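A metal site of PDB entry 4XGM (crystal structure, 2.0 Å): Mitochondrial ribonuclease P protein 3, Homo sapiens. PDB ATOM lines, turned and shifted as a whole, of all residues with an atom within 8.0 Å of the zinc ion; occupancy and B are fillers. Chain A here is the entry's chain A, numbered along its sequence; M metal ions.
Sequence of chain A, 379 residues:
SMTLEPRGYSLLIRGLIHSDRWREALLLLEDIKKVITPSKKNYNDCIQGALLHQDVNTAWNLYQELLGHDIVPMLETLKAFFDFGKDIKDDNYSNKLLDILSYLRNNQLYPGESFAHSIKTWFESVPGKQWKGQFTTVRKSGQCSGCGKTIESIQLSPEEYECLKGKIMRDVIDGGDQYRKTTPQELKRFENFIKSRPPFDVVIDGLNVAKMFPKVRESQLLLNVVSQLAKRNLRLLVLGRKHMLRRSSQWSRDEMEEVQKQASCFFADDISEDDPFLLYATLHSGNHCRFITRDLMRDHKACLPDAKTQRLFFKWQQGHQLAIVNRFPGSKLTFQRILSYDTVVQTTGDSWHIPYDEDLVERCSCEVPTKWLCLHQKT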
ATOM      1  N   LYS A 132       8.421  11.087 -23.346  1.00  0.00           N
ATOM      2  CA  LYS A 132       8.176  11.637 -24.665  1.00  0.00           C
ATOM      3  C   LYS A 132       9.324  11.279 -25.583  1.00  0.00           C
ATOM      4  O   LYS A 132      10.489  11.472 -25.224  1.00  0.00           O
ATOM      5  CB  LYS A 132       7.992  13.149 -24.589  1.00  0.00           C
ATOM      6  CG  LYS A 132       7.711  13.820 -25.924  1.00  0.00           C
ATOM      7  CD  LYS A 132       7.631  15.343 -25.760  1.00  0.00           C
ATOM      8  CE  LYS A 132       7.518  16.062 -27.097  1.00  0.00           C
ATOM      9  NZ  LYS A 132       7.621  17.539 -26.932  1.00  0.00           N
ATOM     10  N   GLN A 134      11.262  11.549 -29.461  1.00  0.00           N
ATOM     11  CA  GLN A 134      11.470  12.308 -30.684  1.00  0.00           C
ATOM     12  C   GLN A 134      12.618  11.715 -31.487  1.00  0.00           C
ATOM     13  O   GLN A 134      13.580  11.207 -30.902  1.00  0.00           O
ATOM     14  CB  GLN A 134      11.773  13.776 -30.387  1.00  0.00           C
ATOM     15  CG  GLN A 134      10.632  14.550 -29.785  1.00  0.00           C
ATOM     16  CD  GLN A 134      10.918  16.032 -29.798  1.00  0.00           C
ATOM     17  OE1 GLN A 134      11.905  16.479 -29.229  1.00  0.00           O
ATOM     18  NE2 GLN A 134      10.072  16.801 -30.477  1.00  0.00           N
ATOM     19  N   THR A 136      15.742  12.514 -33.603  1.00  0.00           N
ATOM     20  CA  THR A 136      16.646  13.646 -33.501  1.00  0.00           C
ATOM     21  C   THR A 136      18.007  13.334 -34.147  1.00  0.00           C
ATOM     22  O   THR A 136      18.249  12.220 -34.621  1.00  0.00           O
ATOM     23  CB  THR A 136      16.898  14.056 -32.022  1.00  0.00           C
ATOM     24  OG1 THR A 136      17.720  13.085 -31.380  1.00  0.00           O
ATOM     25  CG2 THR A 136      15.590  14.177 -31.249  1.00  0.00           C
ATOM     26  N   THR A 137      18.872  14.334 -34.157  1.00  0.00           N
ATOM     27  CA  THR A 137      20.279  14.145 -34.486  1.00  0.00           C
ATOM     28  C   THR A 137      21.085  14.720 -33.330  1.00  0.00           C
ATOM     29  O   THR A 137      20.513  15.266 -32.386  1.00  0.00           O
ATOM     30  CB  THR A 137      20.690  14.850 -35.794  1.00  0.00           C
ATOM     31  OG1 THR A 137      20.457  16.252 -35.650  1.00  0.00           O
ATOM     32  CG2 THR A 137      19.891  14.324 -36.966  1.00  0.00           C
ATOM     33  N   VAL A 138      22.399  14.632 -33.408  1.00  0.00           N
ATOM     34  CA  VAL A 138      23.209  15.182 -32.346  1.00  0.00           C
ATOM     35  C   VAL A 138      24.021  16.310 -32.949  1.00  0.00           C
ATOM     36  O   VAL A 138      24.486  16.200 -34.083  1.00  0.00           O
ATOM     37  CB  VAL A 138      24.117  14.108 -31.696  1.00  0.00           C
ATOM     38  CG1 VAL A 138      25.067  14.743 -30.669  1.00  0.00           C
ATOM     39  CG2 VAL A 138      23.254  13.000 -31.061  1.00  0.00           C
ATOM     40  N   GLN A 143      25.406  17.771 -28.053  1.00  0.00           N
ATOM     41  CA  GLN A 143      24.076  18.037 -27.516  1.00  0.00           C
ATOM     42  C   GLN A 143      22.996  17.469 -28.419  1.00  0.00           C
ATOM     43  O   GLN A 143      22.971  17.761 -29.624  1.00  0.00           O
ATOM     44  CB  GLN A 143      23.877  19.536 -27.313  1.00  0.00           C
ATOM     45  CG  GLN A 143      24.486  20.053 -26.023  1.00  0.00           C
ATOM     46  CD  GLN A 143      25.182  21.389 -26.194  1.00  0.00           C
ATOM     47  OE1 GLN A 143      25.425  21.842 -27.319  1.00  0.00           O
ATOM     48  NE2 GLN A 143      25.499  22.039 -25.082  1.00  0.00           N
ATOM     49  N   CYS A 144      22.099  16.658 -27.838  1.00  0.00           N
ATOM     50  CA  CYS A 144      20.945  16.180 -28.564  1.00  0.00           C
ATOM     51  C   CYS A 144      20.125  17.363 -29.082  1.00  0.00           C
ATOM     52  O   CYS A 144      19.759  18.257 -28.322  1.00  0.00           O
ATOM     53  CB  CYS A 144      20.075  15.285 -27.673  1.00  0.00           C
ATOM     54  SG  CYS A 144      18.527  14.730 -28.439  1.00  0.00           S
ATOM     55  N   SER A 145      19.837  17.352 -30.386  1.00  0.00           N
ATOM     56  CA  SER A 145      19.033  18.399 -31.022  1.00  0.00           C
ATOM     57  C   SER A 145      17.598  18.397 -30.530  1.00  0.00           C
ATOM     58  O   SER A 145      16.832  19.296 -30.861  1.00  0.00           O
ATOM     59  CB  SER A 145      19.054  18.226 -32.542  1.00  0.00           C
ATOM     60  OG  SER A 145      18.353  17.057 -32.924  1.00  0.00           O
ATOM     61  N   GLY A 146      17.222  17.373 -29.769  1.00  0.00           N
ATOM     62  CA  GLY A 146      15.896  17.320 -29.173  1.00  0.00           C
ATOM     63  C   GLY A 146      15.857  17.941 -27.788  1.00  0.00           C
ATOM     64  O   GLY A 146      15.275  19.004 -27.611  1.00  0.00           O
ATOM     65  N   CYS A 147      16.485  17.283 -26.806  1.00  0.00           N
ATOM     66  CA  CYS A 147      16.342  17.692 -25.416  1.00  0.00           C
ATOM     67  C   CYS A 147      17.441  18.608 -24.879  1.00  0.00           C
ATOM     68  O   CYS A 147      17.324  19.130 -23.774  1.00  0.00           O
ATOM     69  CB  CYS A 147      16.246  16.453 -24.513  1.00  0.00           C
ATOM     70  SG  CYS A 147      17.822  15.533 -24.316  1.00  0.00           S
ATOM     71  N   GLY A 148      18.526  18.770 -25.634  1.00  0.00           N
ATOM     72  CA  GLY A 148      19.612  19.619 -25.182  1.00  0.00           C
ATOM     73  C   GLY A 148      20.641  18.959 -24.280  1.00  0.00           C
ATOM     74  O   GLY A 148      21.644  19.582 -23.955  1.00  0.00           O
ATOM     75  N   LYS A 149      20.407  17.710 -23.871  1.00  0.00           N
ATOM     76  CA  LYS A 149      21.401  17.003 -23.061  1.00  0.00           C
ATOM     77  C   LYS A 149      22.642  16.709 -23.880  1.00  0.00           C
ATOM     78  O   LYS A 149      22.579  16.577 -25.096  1.00  0.00           O
ATOM     79  CB  LYS A 149      20.854  15.692 -22.502  1.00  0.00           C
ATOM     80  CG  LYS A 149      19.917  15.833 -21.316  1.00  0.00           C
ATOM     81  CD  LYS A 149      19.641  14.466 -20.683  1.00  0.00           C
ATOM     82  CE  LYS A 149      18.426  14.469 -19.780  1.00  0.00           C
ATOM     83  NZ  LYS A 149      18.634  15.155 -18.481  1.00  0.00           N
ATOM     84  N   THR A 150      23.769  16.594 -23.187  1.00  0.00           N
ATOM     85  CA  THR A 150      25.030  16.189 -23.792  1.00  0.00           C
ATOM     86  C   THR A 150      25.172  14.665 -23.812  1.00  0.00           C
ATOM     87  O   THR A 150      25.029  14.022 -22.778  1.00  0.00           O
ATOM     88  CB  THR A 150      26.219  16.798 -23.029  1.00  0.00           C
ATOM     89  OG1 THR A 150      26.019  18.210 -22.906  1.00  0.00           O
ATOM     90  CG2 THR A 150      27.531  16.516 -23.758  1.00  0.00           C
ATOM     91  N   ILE A 151      25.455  14.117 -24.994  1.00  0.00           N
ATOM     92  CA  ILE A 151      25.631  12.676 -25.180  1.00  0.00           C
ATOM     93  C   ILE A 151      26.909  12.227 -24.471  1.00  0.00           C
ATOM     94  O   ILE A 151      27.851  13.020 -24.360  1.00  0.00           O
ATOM     95  CB  ILE A 151      25.687  12.340 -26.695  1.00  0.00           C
ATOM     96  CG1 ILE A 151      24.364  12.726 -27.390  1.00  0.00           C
ATOM     97  CG2 ILE A 151      26.005  10.882 -26.947  1.00  0.00           C
ATOM     98  CD1 ILE A 151      23.107  12.043 -26.810  1.00  0.00           C
ATOM     99  N   SER A 351      16.337   9.903 -18.972  1.00  0.00           N
ATOM    100  CA  SER A 351      16.404   9.953 -20.424  1.00  0.00           C
ATOM    101  C   SER A 351      17.071   8.706 -20.997  1.00  0.00           C
ATOM    102  O   SER A 351      17.833   8.017 -20.322  1.00  0.00           O
ATOM    103  CB  SER A 351      17.150  11.198 -20.901  1.00  0.00           C
ATOM    104  OG  SER A 351      18.557  11.079 -20.770  1.00  0.00           O
ATOM    105  N   TRP A 352      16.752   8.415 -22.253  1.00  0.00           N
ATOM    106  CA  TRP A 352      17.469   7.426 -23.037  1.00  0.00           C
ATOM    107  C   TRP A 352      17.855   8.088 -24.338  1.00  0.00           C
ATOM    108  O   TRP A 352      17.132   8.949 -24.840  1.00  0.00           O
ATOM    109  CB  TRP A 352      16.620   6.167 -23.298  1.00  0.00           C
ATOM    110  CG  TRP A 352      16.490   5.243 -22.129  1.00  0.00           C
ATOM    111  CD1 TRP A 352      15.587   5.318 -21.099  1.00  0.00           C
ATOM    112  CD2 TRP A 352      17.273   4.068 -21.874  1.00  0.00           C
ATOM    113  NE1 TRP A 352      15.784   4.286 -20.211  1.00  0.00           N
ATOM    114  CE2 TRP A 352      16.803   3.497 -20.671  1.00  0.00           C
ATOM    115  CE3 TRP A 352      18.335   3.439 -22.546  1.00  0.00           C
ATOM    116  CZ2 TRP A 352      17.362   2.345 -20.120  1.00  0.00           C
ATOM    117  CZ3 TRP A 352      18.885   2.286 -21.997  1.00  0.00           C
ATOM    118  CH2 TRP A 352      18.409   1.759 -20.799  1.00  0.00           C
ATOM    119  N   HIS A 353      18.999   7.710 -24.900  1.00  0.00           N
ATOM    120  CA  HIS A 353      19.295   8.095 -26.260  1.00  0.00           C
ATOM    121  C   HIS A 353      19.741   6.846 -27.000  1.00  0.00           C
ATOM    122  O   HIS A 353      20.654   6.140 -26.574  1.00  0.00           O
ATOM    123  CB  HIS A 353      20.346   9.218 -26.303  1.00  0.00           C
ATOM    124  CG  HIS A 353      19.843  10.509 -25.756  1.00  0.00           C
ATOM    125  ND1 HIS A 353      19.744  10.760 -24.409  1.00  0.00           N
ATOM    126  CD2 HIS A 353      19.329  11.603 -26.378  1.00  0.00           C
ATOM    127  CE1 HIS A 353      19.220  11.963 -24.218  1.00  0.00           C
ATOM    128  NE2 HIS A 353      18.978  12.494 -25.401  1.00  0.00           N
ATOM    129  N   ILE A 354      19.051   6.575 -28.093  1.00  0.00           N
ATOM    130  CA  ILE A 354      19.163   5.323 -28.815  1.00  0.00           C
ATOM    131  C   ILE A 354      19.432   5.580 -30.299  1.00  0.00           C
ATOM    132  O   ILE A 354      18.549   6.010 -31.042  1.00  0.00           O
ATOM    133  CB  ILE A 354      17.875   4.481 -28.647  1.00  0.00           C
ATOM    134  CG1 ILE A 354      17.693   4.074 -27.174  1.00  0.00           C
ATOM    135  CG2 ILE A 354      17.925   3.256 -29.529  1.00  0.00           C
ATOM    136  CD1 ILE A 354      16.321   3.419 -26.846  1.00  0.00           C
ATOM    137  N   TRP A 372      19.099   9.449 -34.091  1.00  0.00           N
ATOM    138  CA  TRP A 372      18.870   9.032 -32.726  1.00  0.00           C
ATOM    139  C   TRP A 372      17.381   9.071 -32.389  1.00  0.00           C
ATOM    140  O   TRP A 372      16.612   9.903 -32.899  1.00  0.00           O
ATOM    141  CB  TRP A 372      19.636   9.920 -31.748  1.00  0.00           C
ATOM    142  CG  TRP A 372      21.138   9.799 -31.806  1.00  0.00           C
ATOM    143  CD1 TRP A 372      21.963  10.202 -32.812  1.00  0.00           C
ATOM    144  CD2 TRP A 372      21.983   9.277 -30.781  1.00  0.00           C
ATOM    145  NE1 TRP A 372      23.276   9.955 -32.493  1.00  0.00           N
ATOM    146  CE2 TRP A 372      23.321   9.386 -31.237  1.00  0.00           C
ATOM    147  CE3 TRP A 372      21.757   8.712 -29.516  1.00  0.00           C
ATOM    148  CZ2 TRP A 372      24.408   8.964 -30.483  1.00  0.00           C
ATOM    149  CZ3 TRP A 372      22.854   8.292 -28.760  1.00  0.00           C
ATOM    150  CH2 TRP A 372      24.155   8.415 -29.249  1.00  0.00           C
ATOM    151  N   LEU A 373      16.984   8.155 -31.519  1.00  0.00           N
ATOM    152  CA  LEU A 373      15.714   8.267 -30.815  1.00  0.00           C
ATOM    153  C   LEU A 373      16.024   8.882 -29.462  1.00  0.00           C
ATOM    154  O   LEU A 373      16.834   8.360 -28.694  1.00  0.00           O
ATOM    155  CB  LEU A 373      15.038   6.894 -30.664  1.00  0.00           C
ATOM    156  CG  LEU A 373      13.865   6.789 -29.690  1.00  0.00           C
ATOM    157  CD1 LEU A 373      12.752   7.838 -30.006  1.00  0.00           C
ATOM    158  CD2 LEU A 373      13.290   5.353 -29.712  1.00  0.00           C
ATOM    159  N   CYS A 374      15.369   9.998 -29.183  1.00  0.00           N
ATOM    160  CA  CYS A 374      15.553  10.729 -27.944  1.00  0.00           C
ATOM    161  C   CYS A 374      14.341  10.547 -27.069  1.00  0.00           C
ATOM    162  O   CYS A 374      13.234  10.915 -27.462  1.00  0.00           O
ATOM    163  CB  CYS A 374      15.745  12.233 -28.199  1.00  0.00           C
ATOM    164  SG  CYS A 374      15.408  13.280 -26.740  1.00  0.00           S
ATOM    165  N   LEU A 375      14.530   9.963 -25.893  1.00  0.00           N
ATOM    166  CA  LEU A 375      13.431   9.779 -24.968  1.00  0.00           C
ATOM    167  C   LEU A 375      13.709  10.538 -23.705  1.00  0.00           C
ATOM    168  O   LEU A 375      14.796  10.461 -23.136  1.00  0.00           O
ATOM    169  CB  LEU A 375      13.212   8.302 -24.653  1.00  0.00           C
ATOM    170  CG  LEU A 375      12.765   7.442 -25.831  1.00  0.00           C
ATOM    171  CD1 LEU A 375      13.338   6.011 -25.711  1.00  0.00           C
ATOM    172  CD2 LEU A 375      11.233   7.440 -25.925  1.00  0.00           C
ATOM    173  N   HIS A 376      12.718  11.289 -23.249  1.00  0.00           N
ATOM    174  CA  HIS A 376      12.873  12.083 -22.061  1.00  0.00           C
ATOM    175  C   HIS A 376      11.571  12.103 -21.295  1.00  0.00           C
ATOM    176  O   HIS A 376      10.495  12.150 -21.891  1.00  0.00           O
ATOM    177  CB  HIS A 376      13.319  13.504 -22.427  1.00  0.00           C
ATOM    178  CG  HIS A 376      13.963  14.237 -21.302  1.00  0.00           C
ATOM    179  ND1 HIS A 376      13.244  14.845 -20.297  1.00  0.00           N
ATOM    180  CD2 HIS A 376      15.274  14.466 -21.019  1.00  0.00           C
ATOM    181  CE1 HIS A 376      14.076  15.409 -19.435  1.00  0.00           C
ATOM    182  NE2 HIS A 376      15.308  15.196 -19.852  1.00  0.00           N
HETATM  183 ZN    ZN M   1      17.617  14.088 -26.235  1.00  0.00          ZN
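The backbone carbonyl oxygen of Gln 134 is in hydrogen-bond range of the backbone NH of Cys 374, at 2.8 Å.
N of Lys 149 sits close to SG of Cys 147.
SG of Cys 144 lies close to N of Gly 146 (3.2 Å).
N of Cys 144 sits at hydrogen-bond distance from O of Lys 149.
The side-chain sulfur of Cys 144 sits close to the side-chain hydroxyl of Thr 136 (3.5 Å).
A ring nitrogen (NE2) of His 353 is bound to the zinc ion.
The zinc ion is bound by SG of Cys 374 (2.4 Å).
SG of Cys 147 binds the zinc ion.
SG of Cys 144 is bound to the zinc ion (2.5 Å).
Of the 23 residues printed, 4 come within 4 Å of the zinc ion.
The nearest printed residue that does not touch the zinc ion is Gly 146 (4.5 Å).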
